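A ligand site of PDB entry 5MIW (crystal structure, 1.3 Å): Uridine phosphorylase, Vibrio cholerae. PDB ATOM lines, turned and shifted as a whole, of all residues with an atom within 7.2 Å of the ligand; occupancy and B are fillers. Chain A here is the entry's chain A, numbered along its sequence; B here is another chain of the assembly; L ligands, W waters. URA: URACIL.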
ATOM      1  N   GLY A  92      -5.799 -16.265   5.176  1.00  0.00           N
ATOM      2  CA  GLY A  92      -4.782 -16.246   4.134  1.00  0.00           C
ATOM      3  C   GLY A  92      -3.421 -16.263   4.804  1.00  0.00           C
ATOM      4  O   GLY A  92      -3.332 -16.138   6.018  1.00  0.00           O
ATOM      5  N   THR A  93      -2.352 -16.424   4.009  1.00  0.00           N
ATOM      6  CA  THR A  93      -1.007 -16.382   4.577  1.00  0.00           C
ATOM      7  C   THR A  93      -0.502 -14.954   4.661  1.00  0.00           C
ATOM      8  O   THR A  93      -1.023 -14.038   4.006  1.00  0.00           O
ATOM      9  CB  THR A  93      -0.052 -17.154   3.637  1.00  0.00           C
ATOM     10  OG1 THR A  93      -0.037 -16.498   2.349  1.00  0.00           O
ATOM     11  CG2 THR A  93      -0.513 -18.646   3.511  1.00  0.00           C
ATOM     12  N   THR A  94       0.571 -14.765   5.455  1.00  0.00           N
ATOM     13  CA  THR A  94       1.057 -13.405   5.620  1.00  0.00           C
ATOM     14  C   THR A  94       2.545 -13.428   5.957  1.00  0.00           C
ATOM     15  O   THR A  94       3.061 -14.399   6.515  1.00  0.00           O
ATOM     16  CB  THR A  94       0.230 -12.640   6.655  1.00  0.00           C
ATOM     17  OG1 THR A  94       0.588 -11.249   6.593  1.00  0.00           O
ATOM     18  CG2 THR A  94       0.540 -13.150   8.115  1.00  0.00           C
ATOM     19  N   GLY A  95       3.209 -12.295   5.662  1.00  0.00           N
ATOM     20  CA  GLY A  95       4.600 -12.075   6.077  1.00  0.00           C
ATOM     21  C   GLY A  95       4.610 -11.075   7.215  1.00  0.00           C
ATOM     22  O   GLY A  95       4.064  -9.966   7.068  1.00  0.00           O
ATOM     23  N   ALA A  96       5.164 -11.442   8.378  1.00  0.00           N
ATOM     24  CA  ALA A  96       5.257 -10.505   9.494  1.00  0.00           C
ATOM     25  C   ALA A  96       6.439  -9.573   9.285  1.00  0.00           C
ATOM     26  O   ALA A  96       7.472  -9.948   8.716  1.00  0.00           O
ATOM     27  CB  ALA A  96       5.397 -11.243  10.847  1.00  0.00           C
ATOM     28  N   ILE A  97       6.320  -8.366   9.828  1.00  0.00           N
ATOM     29  CA  ILE A  97       7.407  -7.388   9.746  1.00  0.00           C
ATOM     30  C   ILE A  97       7.878  -6.907  11.106  1.00  0.00           C
ATOM     31  O   ILE A  97       8.772  -6.074  11.178  1.00  0.00           O
ATOM     32  CB  ILE A  97       7.077  -6.200   8.835  1.00  0.00           C
ATOM     33  CG1 ILE A  97       5.934  -5.356   9.428  1.00  0.00           C
ATOM     34  CG2 ILE A  97       6.692  -6.739   7.410  1.00  0.00           C
ATOM     35  CD1 ILE A  97       5.679  -4.070   8.689  1.00  0.00           C
ATOM     36  N   ALA A 156      -0.562  -4.085   6.564  1.00  0.00           N
ATOM     37  CA  ALA A 156      -0.291  -3.344   5.330  1.00  0.00           C
ATOM     38  C   ALA A 156      -0.723  -4.215   4.147  1.00  0.00           C
ATOM     39  O   ALA A 156      -0.247  -5.358   4.007  1.00  0.00           O
ATOM     40  CB  ALA A 156       1.198  -2.999   5.214  1.00  0.00           C
ATOM     41  N   SER A 158      -1.084  -4.718   0.275  1.00  0.00           N
ATOM     42  CA  SER A 158      -0.428  -4.227  -0.935  1.00  0.00           C
ATOM     43  C   SER A 158      -0.927  -4.879  -2.225  1.00  0.00           C
ATOM     44  O   SER A 158      -1.112  -6.105  -2.271  1.00  0.00           O
ATOM     45  CB  SER A 158       1.060  -4.560  -0.788  1.00  0.00           C
ATOM     46  OG  SER A 158       1.796  -4.238  -1.947  1.00  0.00           O
ATOM     47  N   THR A 160       0.968  -5.291  -4.684  1.00  0.00           N
ATOM     48  CA  THR A 160       2.059  -6.129  -5.193  1.00  0.00           C
ATOM     49  C   THR A 160       2.711  -6.971  -4.086  1.00  0.00           C
ATOM     50  O   THR A 160       2.685  -6.630  -2.897  1.00  0.00           O
ATOM     51  CB  THR A 160       3.154  -5.333  -5.918  1.00  0.00           C
ATOM     52  OG1 THR A 160       3.713  -4.336  -5.048  1.00  0.00           O
ATOM     53  CG2 THR A 160       2.592  -4.600  -7.169  1.00  0.00           C
ATOM     54  N   PHE A 161       3.297  -8.102  -4.477  1.00  0.00           N
ATOM     55  CA  PHE A 161       4.129  -8.900  -3.572  1.00  0.00           C
ATOM     56  C   PHE A 161       5.532  -8.329  -3.480  1.00  0.00           C
ATOM     57  O   PHE A 161       6.207  -8.504  -2.451  1.00  0.00           O
ATOM     58  CB  PHE A 161       4.174 -10.327  -4.113  1.00  0.00           C
ATOM     59  CG  PHE A 161       4.800 -11.293  -3.167  1.00  0.00           C
ATOM     60  CD1 PHE A 161       4.079 -11.873  -2.133  1.00  0.00           C
ATOM     61  CD2 PHE A 161       6.161 -11.660  -3.345  1.00  0.00           C
ATOM     62  CE1 PHE A 161       4.675 -12.790  -1.298  1.00  0.00           C
ATOM     63  CE2 PHE A 161       6.753 -12.628  -2.500  1.00  0.00           C
ATOM     64  CZ  PHE A 161       6.023 -13.155  -1.460  1.00  0.00           C
ATOM     65  N   GLN A 165       5.900  -4.367  -1.091  1.00  0.00           N
ATOM     66  CA  GLN A 165       6.377  -4.928   0.167  1.00  0.00           C
ATOM     67  C   GLN A 165       7.862  -4.646   0.332  1.00  0.00           C
ATOM     68  O   GLN A 165       8.536  -5.268   1.173  1.00  0.00           O
ATOM     69  CB  GLN A 165       6.037  -6.428   0.240  1.00  0.00           C
ATOM     70  CG  GLN A 165       4.530  -6.635   0.024  1.00  0.00           C
ATOM     71  CD  GLN A 165       3.998  -8.022   0.371  1.00  0.00           C
ATOM     72  OE1 GLN A 165       4.632  -8.772   1.128  1.00  0.00           O
ATOM     73  NE2 GLN A 165       2.860  -8.369  -0.223  1.00  0.00           N
ATOM     74  N   ARG A 167      10.485  -5.358  -1.493  1.00  0.00           N
ATOM     75  CA  ARG A 167      11.440  -6.413  -1.826  1.00  0.00           C
ATOM     76  C   ARG A 167      12.354  -5.878  -2.915  1.00  0.00           C
ATOM     77  O   ARG A 167      11.871  -5.354  -3.930  1.00  0.00           O
ATOM     78  CB  ARG A 167      10.710  -7.680  -2.321  1.00  0.00           C
ATOM     79  CG  ARG A 167      10.052  -8.421  -1.181  1.00  0.00           C
ATOM     80  CD  ARG A 167       9.441  -9.788  -1.696  1.00  0.00           C
ATOM     81  NE  ARG A 167       9.203 -10.737  -0.593  1.00  0.00           N
ATOM     82  CZ  ARG A 167       8.127 -10.773   0.187  1.00  0.00           C
ATOM     83  NH1 ARG A 167       7.120  -9.957  -0.070  1.00  0.00           N
ATOM     84  NH2 ARG A 167       8.052 -11.615   1.188  1.00  0.00           N
ATOM     85  N   ASN A 193       2.191  -6.794   9.625  1.00  0.00           N
ATOM     86  CA  ASN A 193       2.325  -7.786   8.549  1.00  0.00           C
ATOM     87  C   ASN A 193       1.907  -7.202   7.210  1.00  0.00           C
ATOM     88  O   ASN A 193       1.194  -6.190   7.144  1.00  0.00           O
ATOM     89  CB  ASN A 193       1.444  -9.030   8.834  1.00  0.00           C
ATOM     90  CG  ASN A 193      -0.071  -8.722   8.913  1.00  0.00           C
ATOM     91  OD1 ASN A 193      -0.486  -7.779   9.605  1.00  0.00           O
ATOM     92  ND2 ASN A 193      -0.861  -9.597   8.327  1.00  0.00           N
ATOM     93  N   PHE A 194       2.303  -7.883   6.143  1.00  0.00           N
ATOM     94  CA  PHE A 194       1.890  -7.608   4.772  1.00  0.00           C
ATOM     95  C   PHE A 194       1.054  -8.760   4.214  1.00  0.00           C
ATOM     96  O   PHE A 194       1.365  -9.950   4.425  1.00  0.00           O
ATOM     97  CB  PHE A 194       3.097  -7.603   3.841  1.00  0.00           C
ATOM     98  CG  PHE A 194       3.874  -6.280   3.777  1.00  0.00           C
ATOM     99  CD1 PHE A 194       3.277  -5.138   3.263  1.00  0.00           C
ATOM    100  CD2 PHE A 194       5.241  -6.186   4.199  1.00  0.00           C
ATOM    101  CE1 PHE A 194       3.973  -3.949   3.138  1.00  0.00           C
ATOM    102  CE2 PHE A 194       5.942  -5.003   4.037  1.00  0.00           C
ATOM    103  CZ  PHE A 194       5.281  -3.879   3.509  1.00  0.00           C
ATOM    104  N   GLU A 195      -0.021  -8.412   3.502  1.00  0.00           N
ATOM    105  CA  GLU A 195      -0.729  -9.378   2.656  1.00  0.00           C
ATOM    106  C   GLU A 195      -1.323  -8.543   1.515  1.00  0.00           C
ATOM    107  O   GLU A 195      -0.944  -7.373   1.346  1.00  0.00           O
ATOM    108  CB  GLU A 195      -1.674 -10.273   3.449  1.00  0.00           C
ATOM    109  CG  GLU A 195      -2.647  -9.594   4.341  1.00  0.00           C
ATOM    110  CD  GLU A 195      -3.740  -8.838   3.541  1.00  0.00           C
ATOM    111  OE1 GLU A 195      -3.677  -7.582   3.409  1.00  0.00           O
ATOM    112  OE2 GLU A 195      -4.668  -9.482   2.985  1.00  0.00           O
ATOM    113  N   MET A 196      -2.263  -9.104   0.738  1.00  0.00           N
ATOM    114  CA  MET A 196      -2.607  -8.487  -0.540  1.00  0.00           C
ATOM    115  C   MET A 196      -4.126  -8.373  -0.781  1.00  0.00           C
ATOM    116  O   MET A 196      -4.506  -8.059  -1.929  1.00  0.00           O
ATOM    117  CB  MET A 196      -1.939  -9.175  -1.762  1.00  0.00           C
ATOM    118  CG  MET A 196      -0.416  -9.223  -1.562  1.00  0.00           C
ATOM    119  SD  MET A 196       0.452 -10.016  -2.946  1.00  0.00           S
ATOM    120  CE  MET A 196      -0.137  -9.046  -4.337  1.00  0.00           C
ATOM    121  N   GLU A 197      -5.013  -8.603   0.224  1.00  0.00           N
ATOM    122  CA  GLU A 197      -6.446  -8.585  -0.053  1.00  0.00           C
ATOM    123  C   GLU A 197      -7.263  -7.863   1.005  1.00  0.00           C
ATOM    124  O   GLU A 197      -8.396  -7.455   0.694  1.00  0.00           O
ATOM    125  CB  GLU A 197      -6.961 -10.057  -0.125  1.00  0.00           C
ATOM    126  CG  GLU A 197      -6.455 -10.821  -1.328  1.00  0.00           C
ATOM    127  CD  GLU A 197      -5.057 -11.404  -1.116  1.00  0.00           C
ATOM    128  OE1 GLU A 197      -4.595 -11.566   0.041  1.00  0.00           O
ATOM    129  OE2 GLU A 197      -4.409 -11.710  -2.141  1.00  0.00           O
ATOM    130  N   GLY A 217      -2.230 -16.712   8.967  1.00  0.00           N
ATOM    131  CA  GLY A 217      -1.103 -17.440   9.568  1.00  0.00           C
ATOM    132  C   GLY A 217       0.219 -16.895   9.063  1.00  0.00           C
ATOM    133  O   GLY A 217       0.379 -16.657   7.850  1.00  0.00           O
ATOM    134  N   ILE A 219       3.712 -17.037   7.783  1.00  0.00           N
ATOM    135  CA  ILE A 219       4.526 -18.037   7.107  1.00  0.00           C
ATOM    136  C   ILE A 219       5.964 -17.589   6.938  1.00  0.00           C
ATOM    137  O   ILE A 219       6.844 -18.421   6.651  1.00  0.00           O
ATOM    138  CB  ILE A 219       3.930 -18.457   5.736  1.00  0.00           C
ATOM    139  CG1 ILE A 219       3.992 -17.306   4.703  1.00  0.00           C
ATOM    140  CG2 ILE A 219       2.506 -18.958   5.913  1.00  0.00           C
ATOM    141  CD1 ILE A 219       3.729 -17.773   3.261  1.00  0.00           C
ATOM    142  N   ILE A 220       6.241 -16.299   7.104  1.00  0.00           N
ATOM    143  CA  ILE A 220       7.608 -15.791   7.092  1.00  0.00           C
ATOM    144  C   ILE A 220       7.634 -14.522   7.911  1.00  0.00           C
ATOM    145  O   ILE A 220       6.611 -13.850   8.074  1.00  0.00           O
ATOM    146  CB  ILE A 220       8.031 -15.533   5.623  1.00  0.00           C
ATOM    147  CG1 ILE A 220       9.551 -15.537   5.436  1.00  0.00           C
ATOM    148  CG2 ILE A 220       7.373 -14.313   4.993  1.00  0.00           C
ATOM    149  CD1 ILE A 220       9.906 -15.463   4.023  1.00  0.00           C
ATOM    150  N   ASN A 221       8.817 -14.185   8.416  1.00  0.00           N
ATOM    151  CA  ASN A 221       9.033 -12.933   9.106  1.00  0.00           C
ATOM    152  C   ASN A 221      10.198 -12.259   8.388  1.00  0.00           C
ATOM    153  O   ASN A 221      11.317 -12.795   8.376  1.00  0.00           O
ATOM    154  CB  ASN A 221       9.337 -13.172  10.593  1.00  0.00           C
ATOM    155  CG  ASN A 221       9.496 -11.854  11.343  1.00  0.00           C
ATOM    156  OD1 ASN A 221      10.220 -10.972  10.913  1.00  0.00           O
ATOM    157  ND2 ASN A 221       8.847 -11.729  12.482  1.00  0.00           N
ATOM    158  N   ARG A 222       9.961 -11.076   7.841  1.00  0.00           N
ATOM    159  CA  ARG A 222      10.919 -10.314   7.011  1.00  0.00           C
ATOM    160  C   ARG A 222      12.151  -9.906   7.783  1.00  0.00           C
ATOM    161  O   ARG A 222      13.137  -9.532   7.161  1.00  0.00           O
ATOM    162  CB  ARG A 222      10.235  -9.082   6.444  1.00  0.00           C
ATOM    163  CG  ARG A 222       9.128  -9.442   5.408  1.00  0.00           C
ATOM    164  CD  ARG A 222       9.676  -9.936   4.077  1.00  0.00           C
ATOM    165  NE  ARG A 222      10.547  -8.944   3.396  1.00  0.00           N
ATOM    166  CZ  ARG A 222      10.045  -7.903   2.707  1.00  0.00           C
ATOM    167  NH1 ARG A 222      10.875  -7.010   2.144  1.00  0.00           N
ATOM    168  NH2 ARG A 222       8.716  -7.761   2.523  1.00  0.00           N
ATOM    169  N   PHE B   6       8.725 -18.022  -6.356  1.00  0.00           N
ATOM    170  CA  PHE B   6       7.919 -18.285  -5.172  1.00  0.00           C
ATOM    171  C   PHE B   6       6.514 -18.763  -5.523  1.00  0.00           C
ATOM    172  O   PHE B   6       5.979 -19.659  -4.851  1.00  0.00           O
ATOM    173  CB  PHE B   6       7.839 -17.045  -4.298  1.00  0.00           C
ATOM    174  CG  PHE B   6       7.130 -17.265  -3.000  1.00  0.00           C
ATOM    175  CD1 PHE B   6       5.761 -17.067  -2.895  1.00  0.00           C
ATOM    176  CD2 PHE B   6       7.842 -17.642  -1.871  1.00  0.00           C
ATOM    177  CE1 PHE B   6       5.105 -17.265  -1.705  1.00  0.00           C
ATOM    178  CE2 PHE B   6       7.194 -17.836  -0.675  1.00  0.00           C
ATOM    179  CZ  PHE B   6       5.807 -17.623  -0.597  1.00  0.00           C
ATOM    180  N   HIS B   7       5.893 -18.165  -6.527  1.00  0.00           N
ATOM    181  CA  HIS B   7       4.504 -18.489  -6.841  1.00  0.00           C
ATOM    182  C   HIS B   7       4.349 -19.412  -8.053  1.00  0.00           C
ATOM    183  O   HIS B   7       3.492 -20.290  -8.008  1.00  0.00           O
ATOM    184  CB  HIS B   7       3.679 -17.225  -7.059  1.00  0.00           C
ATOM    185  CG  HIS B   7       3.582 -16.328  -5.862  1.00  0.00           C
ATOM    186  ND1 HIS B   7       4.525 -15.358  -5.577  1.00  0.00           N
ATOM    187  CD2 HIS B   7       2.642 -16.240  -4.880  1.00  0.00           C
ATOM    188  CE1 HIS B   7       4.154 -14.687  -4.478  1.00  0.00           C
ATOM    189  NE2 HIS B   7       3.020 -15.220  -4.030  1.00  0.00           N
ATOM    190  N   ARG B  47      -2.041 -22.088  -7.372  1.00  0.00           N
ATOM    191  CA  ARG B  47      -3.007 -20.981  -7.308  1.00  0.00           C
ATOM    192  C   ARG B  47      -3.606 -20.721  -8.716  1.00  0.00           C
ATOM    193  O   ARG B  47      -3.908 -21.676  -9.443  1.00  0.00           O
ATOM    194  CB  ARG B  47      -2.328 -19.750  -6.662  1.00  0.00           C
ATOM    195  CG  ARG B  47      -2.064 -19.945  -5.140  1.00  0.00           C
ATOM    196  CD  ARG B  47      -1.372 -18.671  -4.601  1.00  0.00           C
ATOM    197  NE  ARG B  47      -1.153 -18.649  -3.141  1.00  0.00           N
ATOM    198  CZ  ARG B  47      -1.894 -17.995  -2.242  1.00  0.00           C
ATOM    199  NH1 ARG B  47      -3.004 -17.288  -2.606  1.00  0.00           N
ATOM    200  NH2 ARG B  47      -1.538 -18.034  -0.954  1.00  0.00           N
HETATM  201  N1  URA L   1       1.897 -13.049   1.685  1.00  0.00           N
HETATM  202  C2  URA L   1       2.320 -11.689   1.356  1.00  0.00           C
HETATM  203  O2  URA L   1       1.644 -10.901   0.809  1.00  0.00           O
HETATM  204  N3  URA L   1       3.641 -11.338   1.815  1.00  0.00           N
HETATM  205  C4  URA L   1       4.554 -12.225   2.423  1.00  0.00           C
HETATM  206  O4  URA L   1       5.652 -11.858   2.757  1.00  0.00           O
HETATM  207  C5  URA L   1       4.082 -13.579   2.719  1.00  0.00           C
HETATM  208  C6  URA L   1       2.795 -13.971   2.306  1.00  0.00           C
HETATM  209  O   HOH W   1       6.355  -9.233   3.321  1.00  0.00           O
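The side-chain amide oxygen (OE1) of Gln 165 lies within hydrogen-bond range of a nitrogen (N3) of the ligand. The guanidinium group of Arg 167 sits at hydrogen-bond distance from an oxygen (O4) of the ligand (2.9 Å).
The backbone carbonyl oxygen of Gln 165 is in hydrogen-bond range of the guanidinium group of Arg 222, at 2.8 Å. NE2 of Gln 165 lies within hydrogen-bond range of O of Thr 160 (3.2 Å). The guanidinium group of Arg 167 lies within hydrogen-bond range of the backbone carbonyl oxygen of Phe 161, at 2.9 Å. The side-chain carboxylate of Glu 195 lies within hydrogen-bond range of the backbone NH of Glu 197 (2.9 Å). O of Glu 195 lies within hydrogen-bond range of N of Ser 158 (2.9 Å). The side-chain hydroxyl of Thr 94 lies within hydrogen-bond range of the backbone carbonyl oxygen of Phe 194, at 2.6 Å. O of Thr 94 is in hydrogen-bond range of N of Ile 219. ND2 of Asn 193 lies within hydrogen-bond range of OG1 of Thr 94 (2.8 Å).
Thr 93 touches the ligand (OG1 to C6, 3.8 Å). Thr 94 touches the ligand (C to C5, 3.6 Å). Gly 95 touches the ligand (N to C5, 3.3 Å). CE1 of Phe 161 touches N3 of the ligand (3.6 Å). O of Phe 194 touches C2 of the ligand, 3.7 Å away. Glu 195 touches the ligand. Met 196 touches the ligand (CG to O2, 3.6 Å). Ile 220 touches the ligand (CG2 to O4, 3.7 Å). Hydrophobic or aromatic side chains that line the ligand: Phe 161, Met 196 and Ile 220.
Water W1 lies within hydrogen-bond range of O4 of the ligand (2.8 Å), OE1 of Gln 165 (2.8 Å) and NH2 of Arg 222 (2.9 Å).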
